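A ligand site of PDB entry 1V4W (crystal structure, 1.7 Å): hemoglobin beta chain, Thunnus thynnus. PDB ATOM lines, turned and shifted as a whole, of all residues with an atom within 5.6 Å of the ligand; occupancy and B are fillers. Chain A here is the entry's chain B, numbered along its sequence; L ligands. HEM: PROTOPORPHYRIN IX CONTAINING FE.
A ring nitrogen (NE2) of His 92 is bound to an iron atom (FE) of the ligand, at 2.2 Å.
The side-chain hydroxyl (OH) of Tyr 45 lies within hydrogen-bond range of an oxygen (O2D) of the ligand (2.5 Å).
A ring nitrogen (ND1) of His 92 is in hydrogen-bond range of the backbone carbonyl oxygen of Leu 88 (2.8 Å).
O of His 92 is in hydrogen-bond range of N of Val 98, at 2.9 Å.
The side-chain amide nitrogen (ND2) of Asn 102 is in hydrogen-bond range of the side-chain hydroxyl (OH) of Tyr 41, at 3.5 Å.
N of Leu 96 sits at hydrogen-bond distance from O of Leu 91.
The backbone carbonyl oxygen of Cys 31 is in hydrogen-bond range of the side-chain hydroxyl of Thr 38 (3.4 Å).
The backbone carbonyl oxygen (O) of Gly 70 sits at hydrogen-bond distance from the side-chain hydroxyl (OH) of Tyr 85 (2.7 Å).
NE2 of His 63 sits close to ND of the ligand, 3.3 Å away.
Merely in contact with the ligand: Thr 38 (3.7 Å), Tyr 41 (3.6 Å), Phe 42 (3.8 Å), Lys 66 (3.7 Å), Val 67 (3.6 Å), Gly 70 (3.9 Å), Leu 88 (3.7 Å), Leu 91 (3.5 Å), Leu 96 (3.5 Å), Val 98 (3.9 Å), Asn 102 (3.4 Å), Phe 103 (3.5 Å), Leu 106 (3.98 Å) and Leu 141 (3.7 Å).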
ATOM      1  N   LEU A  28       3.959 -21.554  -8.107  1.00  0.00           N
ATOM      2  CA  LEU A  28       2.627 -22.027  -7.689  1.00  0.00           C
ATOM      3  C   LEU A  28       1.862 -22.572  -8.869  1.00  0.00           C
ATOM      4  O   LEU A  28       1.223 -23.621  -8.744  1.00  0.00           O
ATOM      5  CB  LEU A  28       1.829 -20.944  -6.949  1.00  0.00           C
ATOM      6  CG  LEU A  28       0.482 -21.437  -6.382  1.00  0.00           C
ATOM      7  CD1 LEU A  28       0.649 -22.569  -5.372  1.00  0.00           C
ATOM      8  CD2 LEU A  28      -0.281 -20.271  -5.705  1.00  0.00           C
ATOM      9  N   CYS A  31       3.052 -25.945  -9.722  1.00  0.00           N
ATOM     10  CA  CYS A  31       2.543 -26.900  -8.742  1.00  0.00           C
ATOM     11  C   CYS A  31       1.095 -27.337  -9.067  1.00  0.00           C
ATOM     12  O   CYS A  31       0.802 -28.543  -9.044  1.00  0.00           O
ATOM     13  CB  CYS A  31       2.621 -26.245  -7.370  1.00  0.00           C
ATOM     14  SG  CYS A  31       2.200 -27.397  -6.036  1.00  0.00           S
ATOM     15  N   LEU A  32       0.225 -26.388  -9.396  1.00  0.00           N
ATOM     16  CA  LEU A  32      -1.166 -26.695  -9.692  1.00  0.00           C
ATOM     17  C   LEU A  32      -1.343 -27.496 -10.971  1.00  0.00           C
ATOM     18  O   LEU A  32      -2.293 -28.271 -11.106  1.00  0.00           O
ATOM     19  CB  LEU A  32      -1.958 -25.418  -9.826  1.00  0.00           C
ATOM     20  CG  LEU A  32      -2.580 -24.888  -8.519  1.00  0.00           C
ATOM     21  CD1 LEU A  32      -1.670 -24.888  -7.347  1.00  0.00           C
ATOM     22  CD2 LEU A  32      -3.066 -23.463  -8.800  1.00  0.00           C
ATOM     23  N   THR A  38      -3.524 -30.278  -5.843  1.00  0.00           N
ATOM     24  CA  THR A  38      -3.314 -29.068  -5.052  1.00  0.00           C
ATOM     25  C   THR A  38      -4.343 -28.005  -5.403  1.00  0.00           C
ATOM     26  O   THR A  38      -4.476 -27.033  -4.680  1.00  0.00           O
ATOM     27  CB  THR A  38      -1.893 -28.489  -5.198  1.00  0.00           C
ATOM     28  OG1 THR A  38      -1.598 -28.296  -6.593  1.00  0.00           O
ATOM     29  CG2 THR A  38      -0.820 -29.466  -4.673  1.00  0.00           C
ATOM     30  N   TYR A  41      -7.551 -26.557  -2.935  1.00  0.00           N
ATOM     31  CA  TYR A  41      -7.584 -25.446  -1.977  1.00  0.00           C
ATOM     32  C   TYR A  41      -7.975 -24.112  -2.567  1.00  0.00           C
ATOM     33  O   TYR A  41      -8.153 -23.118  -1.815  1.00  0.00           O
ATOM     34  CB  TYR A  41      -6.228 -25.308  -1.259  1.00  0.00           C
ATOM     35  CG  TYR A  41      -5.818 -26.613  -0.691  1.00  0.00           C
ATOM     36  CD1 TYR A  41      -6.459 -27.119   0.434  1.00  0.00           C
ATOM     37  CD2 TYR A  41      -4.850 -27.397  -1.318  1.00  0.00           C
ATOM     38  CE1 TYR A  41      -6.122 -28.351   0.957  1.00  0.00           C
ATOM     39  CE2 TYR A  41      -4.508 -28.640  -0.825  1.00  0.00           C
ATOM     40  CZ  TYR A  41      -5.150 -29.098   0.334  1.00  0.00           C
ATOM     41  OH  TYR A  41      -4.825 -30.334   0.804  1.00  0.00           O
ATOM     42  N   PHE A  42      -8.132 -24.079  -3.876  1.00  0.00           N
ATOM     43  CA  PHE A  42      -8.207 -22.811  -4.597  1.00  0.00           C
ATOM     44  C   PHE A  42      -9.509 -22.742  -5.365  1.00  0.00           C
ATOM     45  O   PHE A  42      -9.589 -22.097  -6.418  1.00  0.00           O
ATOM     46  CB  PHE A  42      -6.977 -22.687  -5.508  1.00  0.00           C
ATOM     47  CG  PHE A  42      -5.690 -22.616  -4.715  1.00  0.00           C
ATOM     48  CD1 PHE A  42      -5.351 -21.446  -4.055  1.00  0.00           C
ATOM     49  CD2 PHE A  42      -4.845 -23.731  -4.632  1.00  0.00           C
ATOM     50  CE1 PHE A  42      -4.174 -21.362  -3.265  1.00  0.00           C
ATOM     51  CE2 PHE A  42      -3.669 -23.671  -3.871  1.00  0.00           C
ATOM     52  CZ  PHE A  42      -3.328 -22.501  -3.186  1.00  0.00           C
ATOM     53  N   TYR A  45     -10.779 -19.309  -6.451  1.00  0.00           N
ATOM     54  CA  TYR A  45      -9.802 -18.513  -7.166  1.00  0.00           C
ATOM     55  C   TYR A  45     -10.123 -18.361  -8.640  1.00  0.00           C
ATOM     56  O   TYR A  45      -9.382 -17.711  -9.358  1.00  0.00           O
ATOM     57  CB  TYR A  45      -8.402 -19.122  -7.000  1.00  0.00           C
ATOM     58  CG  TYR A  45      -7.751 -18.692  -5.697  1.00  0.00           C
ATOM     59  CD1 TYR A  45      -8.330 -19.021  -4.460  1.00  0.00           C
ATOM     60  CD2 TYR A  45      -6.583 -17.944  -5.696  1.00  0.00           C
ATOM     61  CE1 TYR A  45      -7.741 -18.619  -3.263  1.00  0.00           C
ATOM     62  CE2 TYR A  45      -5.980 -17.541  -4.504  1.00  0.00           C
ATOM     63  CZ  TYR A  45      -6.575 -17.855  -3.302  1.00  0.00           C
ATOM     64  OH  TYR A  45      -5.990 -17.460  -2.117  1.00  0.00           O
ATOM     65  N   HIS A  63      -1.192 -15.139  -4.939  1.00  0.00           N
ATOM     66  CA  HIS A  63      -0.957 -16.075  -3.855  1.00  0.00           C
ATOM     67  C   HIS A  63       0.477 -16.626  -3.896  1.00  0.00           C
ATOM     68  O   HIS A  63       1.096 -16.821  -2.857  1.00  0.00           O
ATOM     69  CB  HIS A  63      -1.987 -17.199  -3.833  1.00  0.00           C
ATOM     70  CG  HIS A  63      -1.917 -17.975  -2.576  1.00  0.00           C
ATOM     71  ND1 HIS A  63      -2.085 -17.364  -1.356  1.00  0.00           N
ATOM     72  CD2 HIS A  63      -1.587 -19.265  -2.320  1.00  0.00           C
ATOM     73  CE1 HIS A  63      -1.900 -18.256  -0.401  1.00  0.00           C
ATOM     74  NE2 HIS A  63      -1.609 -19.415  -0.956  1.00  0.00           N
ATOM     75  N   LYS A  66       2.685 -14.277  -2.230  1.00  0.00           N
ATOM     76  CA  LYS A  66       2.511 -14.346  -0.782  1.00  0.00           C
ATOM     77  C   LYS A  66       3.224 -15.550  -0.152  1.00  0.00           C
ATOM     78  O   LYS A  66       3.844 -15.448   0.899  1.00  0.00           O
ATOM     79  CB  LYS A  66       1.016 -14.409  -0.479  1.00  0.00           C
ATOM     80  CG  LYS A  66       0.678 -14.204   0.983  1.00  0.00           C
ATOM     81  CD  LYS A  66      -0.865 -14.302   1.155  1.00  0.00           C
ATOM     82  CE  LYS A  66      -1.549 -12.988   0.823  1.00  0.00           C
ATOM     83  NZ  LYS A  66      -1.766 -12.806  -0.651  1.00  0.00           N
ATOM     84  N   VAL A  67       3.054 -16.705  -0.786  1.00  0.00           N
ATOM     85  CA  VAL A  67       3.695 -17.918  -0.342  1.00  0.00           C
ATOM     86  C   VAL A  67       5.222 -17.778  -0.348  1.00  0.00           C
ATOM     87  O   VAL A  67       5.906 -18.154   0.587  1.00  0.00           O
ATOM     88  CB  VAL A  67       3.208 -19.111  -1.224  1.00  0.00           C
ATOM     89  CG1 VAL A  67       4.048 -20.313  -0.970  1.00  0.00           C
ATOM     90  CG2 VAL A  67       1.762 -19.406  -0.867  1.00  0.00           C
ATOM     91  N   GLY A  70       6.385 -15.820   2.270  1.00  0.00           N
ATOM     92  CA  GLY A  70       6.306 -16.675   3.436  1.00  0.00           C
ATOM     93  C   GLY A  70       7.634 -17.306   3.837  1.00  0.00           C
ATOM     94  O   GLY A  70       7.827 -17.657   5.008  1.00  0.00           O
ATOM     95  N   LEU A  71       8.565 -17.417   2.891  1.00  0.00           N
ATOM     96  CA  LEU A  71       9.898 -17.944   3.162  1.00  0.00           C
ATOM     97  C   LEU A  71      10.831 -16.921   3.790  1.00  0.00           C
ATOM     98  O   LEU A  71      11.862 -17.299   4.328  1.00  0.00           O
ATOM     99  CB  LEU A  71      10.535 -18.518   1.899  1.00  0.00           C
ATOM    100  CG  LEU A  71       9.826 -19.769   1.404  1.00  0.00           C
ATOM    101  CD1 LEU A  71      10.544 -20.233   0.106  1.00  0.00           C
ATOM    102  CD2 LEU A  71       9.860 -20.852   2.458  1.00  0.00           C
ATOM    103  N   ARG A  73      10.709 -15.163   6.429  1.00  0.00           N
ATOM    104  CA  ARG A  73      10.966 -15.240   7.861  1.00  0.00           C
ATOM    105  C   ARG A  73      12.008 -16.293   8.170  1.00  0.00           C
ATOM    106  O   ARG A  73      12.769 -16.135   9.127  1.00  0.00           O
ATOM    107  CB  ARG A  73       9.684 -15.436   8.660  1.00  0.00           C
ATOM    108  CG  ARG A  73       9.072 -16.792   8.569  1.00  0.00           C
ATOM    109  CD  ARG A  73       7.604 -16.816   9.027  1.00  0.00           C
ATOM    110  NE  ARG A  73       6.731 -16.061   8.133  1.00  0.00           N
ATOM    111  CZ  ARG A  73       5.477 -15.705   8.414  1.00  0.00           C
ATOM    112  NH1 ARG A  73       4.933 -16.053   9.582  1.00  0.00           N
ATOM    113  NH2 ARG A  73       4.749 -15.025   7.536  1.00  0.00           N
ATOM    114  N   TYR A  85       7.665 -20.485  12.237  1.00  0.00           N
ATOM    115  CA  TYR A  85       6.570 -21.076  11.465  1.00  0.00           C
ATOM    116  C   TYR A  85       5.445 -21.690  12.286  1.00  0.00           C
ATOM    117  O   TYR A  85       4.450 -22.166  11.721  1.00  0.00           O
ATOM    118  CB  TYR A  85       7.118 -22.125  10.493  1.00  0.00           C
ATOM    119  CG  TYR A  85       7.769 -21.429   9.333  1.00  0.00           C
ATOM    120  CD1 TYR A  85       9.148 -21.234   9.316  1.00  0.00           C
ATOM    121  CD2 TYR A  85       6.997 -20.863   8.346  1.00  0.00           C
ATOM    122  CE1 TYR A  85       9.759 -20.533   8.250  1.00  0.00           C
ATOM    123  CE2 TYR A  85       7.592 -20.154   7.281  1.00  0.00           C
ATOM    124  CZ  TYR A  85       8.970 -20.038   7.239  1.00  0.00           C
ATOM    125  OH  TYR A  85       9.522 -19.332   6.198  1.00  0.00           O
ATOM    126  N   LEU A  88       2.034 -20.185  11.371  1.00  0.00           N
ATOM    127  CA  LEU A  88       1.673 -20.589  10.015  1.00  0.00           C
ATOM    128  C   LEU A  88       1.379 -22.078   9.952  1.00  0.00           C
ATOM    129  O   LEU A  88       0.541 -22.486   9.149  1.00  0.00           O
ATOM    130  CB  LEU A  88       2.811 -20.282   9.041  1.00  0.00           C
ATOM    131  CG  LEU A  88       2.437 -19.797   7.646  1.00  0.00           C
ATOM    132  CD1 LEU A  88       1.397 -18.674   7.633  1.00  0.00           C
ATOM    133  CD2 LEU A  88       3.733 -19.331   6.944  1.00  0.00           C
ATOM    134  N   LEU A  91      -2.162 -22.372  11.222  1.00  0.00           N
ATOM    135  CA  LEU A  91      -3.026 -21.906  10.168  1.00  0.00           C
ATOM    136  C   LEU A  91      -3.302 -22.983   9.098  1.00  0.00           C
ATOM    137  O   LEU A  91      -4.432 -23.235   8.703  1.00  0.00           O
ATOM    138  CB  LEU A  91      -2.401 -20.669   9.486  1.00  0.00           C
ATOM    139  CG  LEU A  91      -3.286 -20.125   8.365  1.00  0.00           C
ATOM    140  CD1 LEU A  91      -4.554 -19.522   8.896  1.00  0.00           C
ATOM    141  CD2 LEU A  91      -2.537 -19.090   7.570  1.00  0.00           C
ATOM    142  N   HIS A  92      -2.238 -23.560   8.580  1.00  0.00           N
ATOM    143  CA  HIS A  92      -2.419 -24.503   7.500  1.00  0.00           C
ATOM    144  C   HIS A  92      -3.091 -25.785   7.972  1.00  0.00           C
ATOM    145  O   HIS A  92      -3.828 -26.380   7.215  1.00  0.00           O
ATOM    146  CB  HIS A  92      -1.071 -24.825   6.888  1.00  0.00           C
ATOM    147  CG  HIS A  92      -0.598 -23.742   5.970  1.00  0.00           C
ATOM    148  ND1 HIS A  92       0.014 -22.604   6.422  1.00  0.00           N
ATOM    149  CD2 HIS A  92      -0.713 -23.612   4.621  1.00  0.00           C
ATOM    150  CE1 HIS A  92       0.300 -21.811   5.393  1.00  0.00           C
ATOM    151  NE2 HIS A  92      -0.138 -22.399   4.291  1.00  0.00           N
ATOM    152  N   LEU A  96      -6.913 -24.079   7.333  1.00  0.00           N
ATOM    153  CA  LEU A  96      -6.909 -24.360   5.915  1.00  0.00           C
ATOM    154  C   LEU A  96      -7.007 -25.839   5.557  1.00  0.00           C
ATOM    155  O   LEU A  96      -7.403 -26.174   4.443  1.00  0.00           O
ATOM    156  CB  LEU A  96      -5.640 -23.762   5.279  1.00  0.00           C
ATOM    157  CG  LEU A  96      -5.503 -22.235   5.458  1.00  0.00           C
ATOM    158  CD1 LEU A  96      -4.146 -21.754   4.910  1.00  0.00           C
ATOM    159  CD2 LEU A  96      -6.668 -21.548   4.732  1.00  0.00           C
ATOM    160  N   VAL A  98      -4.670 -27.926   4.908  1.00  0.00           N
ATOM    161  CA  VAL A  98      -3.815 -28.264   3.764  1.00  0.00           C
ATOM    162  C   VAL A  98      -2.979 -29.501   4.096  1.00  0.00           C
ATOM    163  O   VAL A  98      -2.312 -29.578   5.116  1.00  0.00           O
ATOM    164  CB  VAL A  98      -2.867 -27.077   3.439  1.00  0.00           C
ATOM    165  CG1 VAL A  98      -1.847 -27.490   2.378  1.00  0.00           C
ATOM    166  CG2 VAL A  98      -3.703 -25.907   2.892  1.00  0.00           C
ATOM    167  N   ASN A 102       1.856 -31.463   0.506  1.00  0.00           N
ATOM    168  CA  ASN A 102       1.887 -30.457  -0.564  1.00  0.00           C
ATOM    169  C   ASN A 102       2.979 -29.418  -0.379  1.00  0.00           C
ATOM    170  O   ASN A 102       3.368 -28.798  -1.354  1.00  0.00           O
ATOM    171  CB  ASN A 102       0.549 -29.791  -0.689  1.00  0.00           C
ATOM    172  CG  ASN A 102      -0.468 -30.756  -1.202  1.00  0.00           C
ATOM    173  OD1 ASN A 102      -0.175 -31.549  -2.088  1.00  0.00           O
ATOM    174  ND2 ASN A 102      -1.681 -30.687  -0.671  1.00  0.00           N
ATOM    175  N   PHE A 103       3.478 -29.279   0.842  1.00  0.00           N
ATOM    176  CA  PHE A 103       4.566 -28.354   1.078  1.00  0.00           C
ATOM    177  C   PHE A 103       5.827 -28.887   0.397  1.00  0.00           C
ATOM    178  O   PHE A 103       6.588 -28.105  -0.230  1.00  0.00           O
ATOM    179  CB  PHE A 103       4.856 -28.180   2.552  1.00  0.00           C
ATOM    180  CG  PHE A 103       3.696 -27.645   3.356  1.00  0.00           C
ATOM    181  CD1 PHE A 103       3.475 -28.133   4.638  1.00  0.00           C
ATOM    182  CD2 PHE A 103       2.852 -26.650   2.853  1.00  0.00           C
ATOM    183  CE1 PHE A 103       2.411 -27.620   5.405  1.00  0.00           C
ATOM    184  CE2 PHE A 103       1.824 -26.130   3.637  1.00  0.00           C
ATOM    185  CZ  PHE A 103       1.600 -26.649   4.903  1.00  0.00           C
ATOM    186  N   LEU A 106       5.423 -28.363  -3.392  1.00  0.00           N
ATOM    187  CA  LEU A 106       5.676 -26.983  -3.774  1.00  0.00           C
ATOM    188  C   LEU A 106       7.172 -26.686  -3.734  1.00  0.00           C
ATOM    189  O   LEU A 106       7.667 -25.989  -4.651  1.00  0.00           O
ATOM    190  CB  LEU A 106       4.919 -26.056  -2.843  1.00  0.00           C
ATOM    191  CG  LEU A 106       4.410 -24.728  -3.423  1.00  0.00           C
ATOM    192  CD1 LEU A 106       4.529 -23.609  -2.388  1.00  0.00           C
ATOM    193  CD2 LEU A 106       4.724 -24.294  -4.816  1.00  0.00           C
ATOM    194  N   VAL A 137      12.259 -25.948   6.373  1.00  0.00           N
ATOM    195  CA  VAL A 137      11.052 -25.161   6.341  1.00  0.00           C
ATOM    196  C   VAL A 137       9.845 -26.081   6.250  1.00  0.00           C
ATOM    197  O   VAL A 137       8.864 -25.882   6.960  1.00  0.00           O
ATOM    198  CB  VAL A 137      11.064 -24.173   5.162  1.00  0.00           C
ATOM    199  CG1 VAL A 137       9.662 -23.564   4.971  1.00  0.00           C
ATOM    200  CG2 VAL A 137      12.120 -23.124   5.394  1.00  0.00           C
ATOM    201  N   LEU A 141       6.746 -26.321   8.897  1.00  0.00           N
ATOM    202  CA  LEU A 141       5.369 -26.088   8.543  1.00  0.00           C
ATOM    203  C   LEU A 141       4.492 -27.260   8.936  1.00  0.00           C
ATOM    204  O   LEU A 141       3.265 -27.077   9.081  1.00  0.00           O
ATOM    205  CB  LEU A 141       5.215 -25.835   7.035  1.00  0.00           C
ATOM    206  CG  LEU A 141       5.590 -24.411   6.647  1.00  0.00           C
ATOM    207  CD1 LEU A 141       5.774 -24.372   5.120  1.00  0.00           C
ATOM    208  CD2 LEU A 141       4.475 -23.483   7.101  1.00  0.00           C
HETATM  209  CHA HEM L   1      -1.998 -18.959   3.035  1.00  0.00           C
HETATM  210  CHB HEM L   1       2.832 -19.538   3.326  1.00  0.00           C
HETATM  211  CHC HEM L   1       2.458 -23.759   1.004  1.00  0.00           C
HETATM  212  CHD HEM L   1      -2.331 -23.128   0.464  1.00  0.00           C
HETATM  213  C1A HEM L   1      -0.665 -18.736   3.276  1.00  0.00           C
HETATM  214  C2A HEM L   1      -0.088 -17.532   3.831  1.00  0.00           C
HETATM  215  C3A HEM L   1       1.234 -17.722   3.924  1.00  0.00           C
HETATM  216  C4A HEM L   1       1.550 -19.010   3.394  1.00  0.00           C
HETATM  217  CMA HEM L   1       2.334 -16.742   4.418  1.00  0.00           C
HETATM  218  CAA HEM L   1      -0.911 -16.281   4.268  1.00  0.00           C
HETATM  219  CBA HEM L   1      -1.155 -16.402   5.775  1.00  0.00           C
HETATM  220  CGA HEM L   1      -1.836 -15.160   6.335  1.00  0.00           C
HETATM  221  O1A HEM L   1      -2.558 -14.464   5.572  1.00  0.00           O
HETATM  222  O2A HEM L   1      -1.638 -14.855   7.540  1.00  0.00           O
HETATM  223  C1B HEM L   1       3.162 -20.747   2.759  1.00  0.00           C
HETATM  224  C2B HEM L   1       4.483 -21.302   2.625  1.00  0.00           C
HETATM  225  C3B HEM L   1       4.369 -22.485   1.970  1.00  0.00           C
HETATM  226  C4B HEM L   1       2.959 -22.688   1.694  1.00  0.00           C
HETATM  227  CMB HEM L   1       5.771 -20.613   3.181  1.00  0.00           C
HETATM  228  CAB HEM L   1       5.429 -23.510   1.560  1.00  0.00           C
HETATM  229  CBB HEM L   1       6.666 -23.076   1.277  1.00  0.00           C
HETATM  230  C1C HEM L   1       1.128 -23.933   0.611  1.00  0.00           C
HETATM  231  C2C HEM L   1       0.625 -24.961  -0.267  1.00  0.00           C
HETATM  232  C3C HEM L   1      -0.685 -24.769  -0.365  1.00  0.00           C
HETATM  233  C4C HEM L   1      -1.044 -23.619   0.400  1.00  0.00           C
HETATM  234  CMC HEM L   1       1.421 -26.088  -0.926  1.00  0.00           C
HETATM  235  CAC HEM L   1      -1.750 -25.538  -1.154  1.00  0.00           C
HETATM  236  CBC HEM L   1      -1.458 -26.412  -2.122  1.00  0.00           C
HETATM  237  C1D HEM L   1      -2.648 -21.924   1.063  1.00  0.00           C
HETATM  238  C2D HEM L   1      -3.975 -21.376   1.102  1.00  0.00           C
HETATM  239  C3D HEM L   1      -3.867 -20.110   1.883  1.00  0.00           C
HETATM  240  C4D HEM L   1      -2.497 -20.002   2.279  1.00  0.00           C
HETATM  241  CMD HEM L   1      -5.238 -21.955   0.448  1.00  0.00           C
HETATM  242  CAD HEM L   1      -5.031 -19.147   2.185  1.00  0.00           C
HETATM  243  CBD HEM L   1      -5.256 -18.322   0.938  1.00  0.00           C
HETATM  244  CGD HEM L   1      -6.545 -17.540   1.085  1.00  0.00           C
HETATM  245  O1D HEM L   1      -6.872 -17.083   2.206  1.00  0.00           O
HETATM  246  O2D HEM L   1      -7.236 -17.350   0.057  1.00  0.00           O
HETATM  247  NA  HEM L   1       0.362 -19.617   3.019  1.00  0.00           N
HETATM  248  NB  HEM L   1       2.268 -21.607   2.200  1.00  0.00           N
HETATM  249  NC  HEM L   1       0.092 -23.107   0.983  1.00  0.00           N
HETATM  250  ND  HEM L   1      -1.795 -21.134   1.805  1.00  0.00           N
HETATM  251 FE   HEM L   1       0.167 -21.514   2.295  1.00  0.00          FE
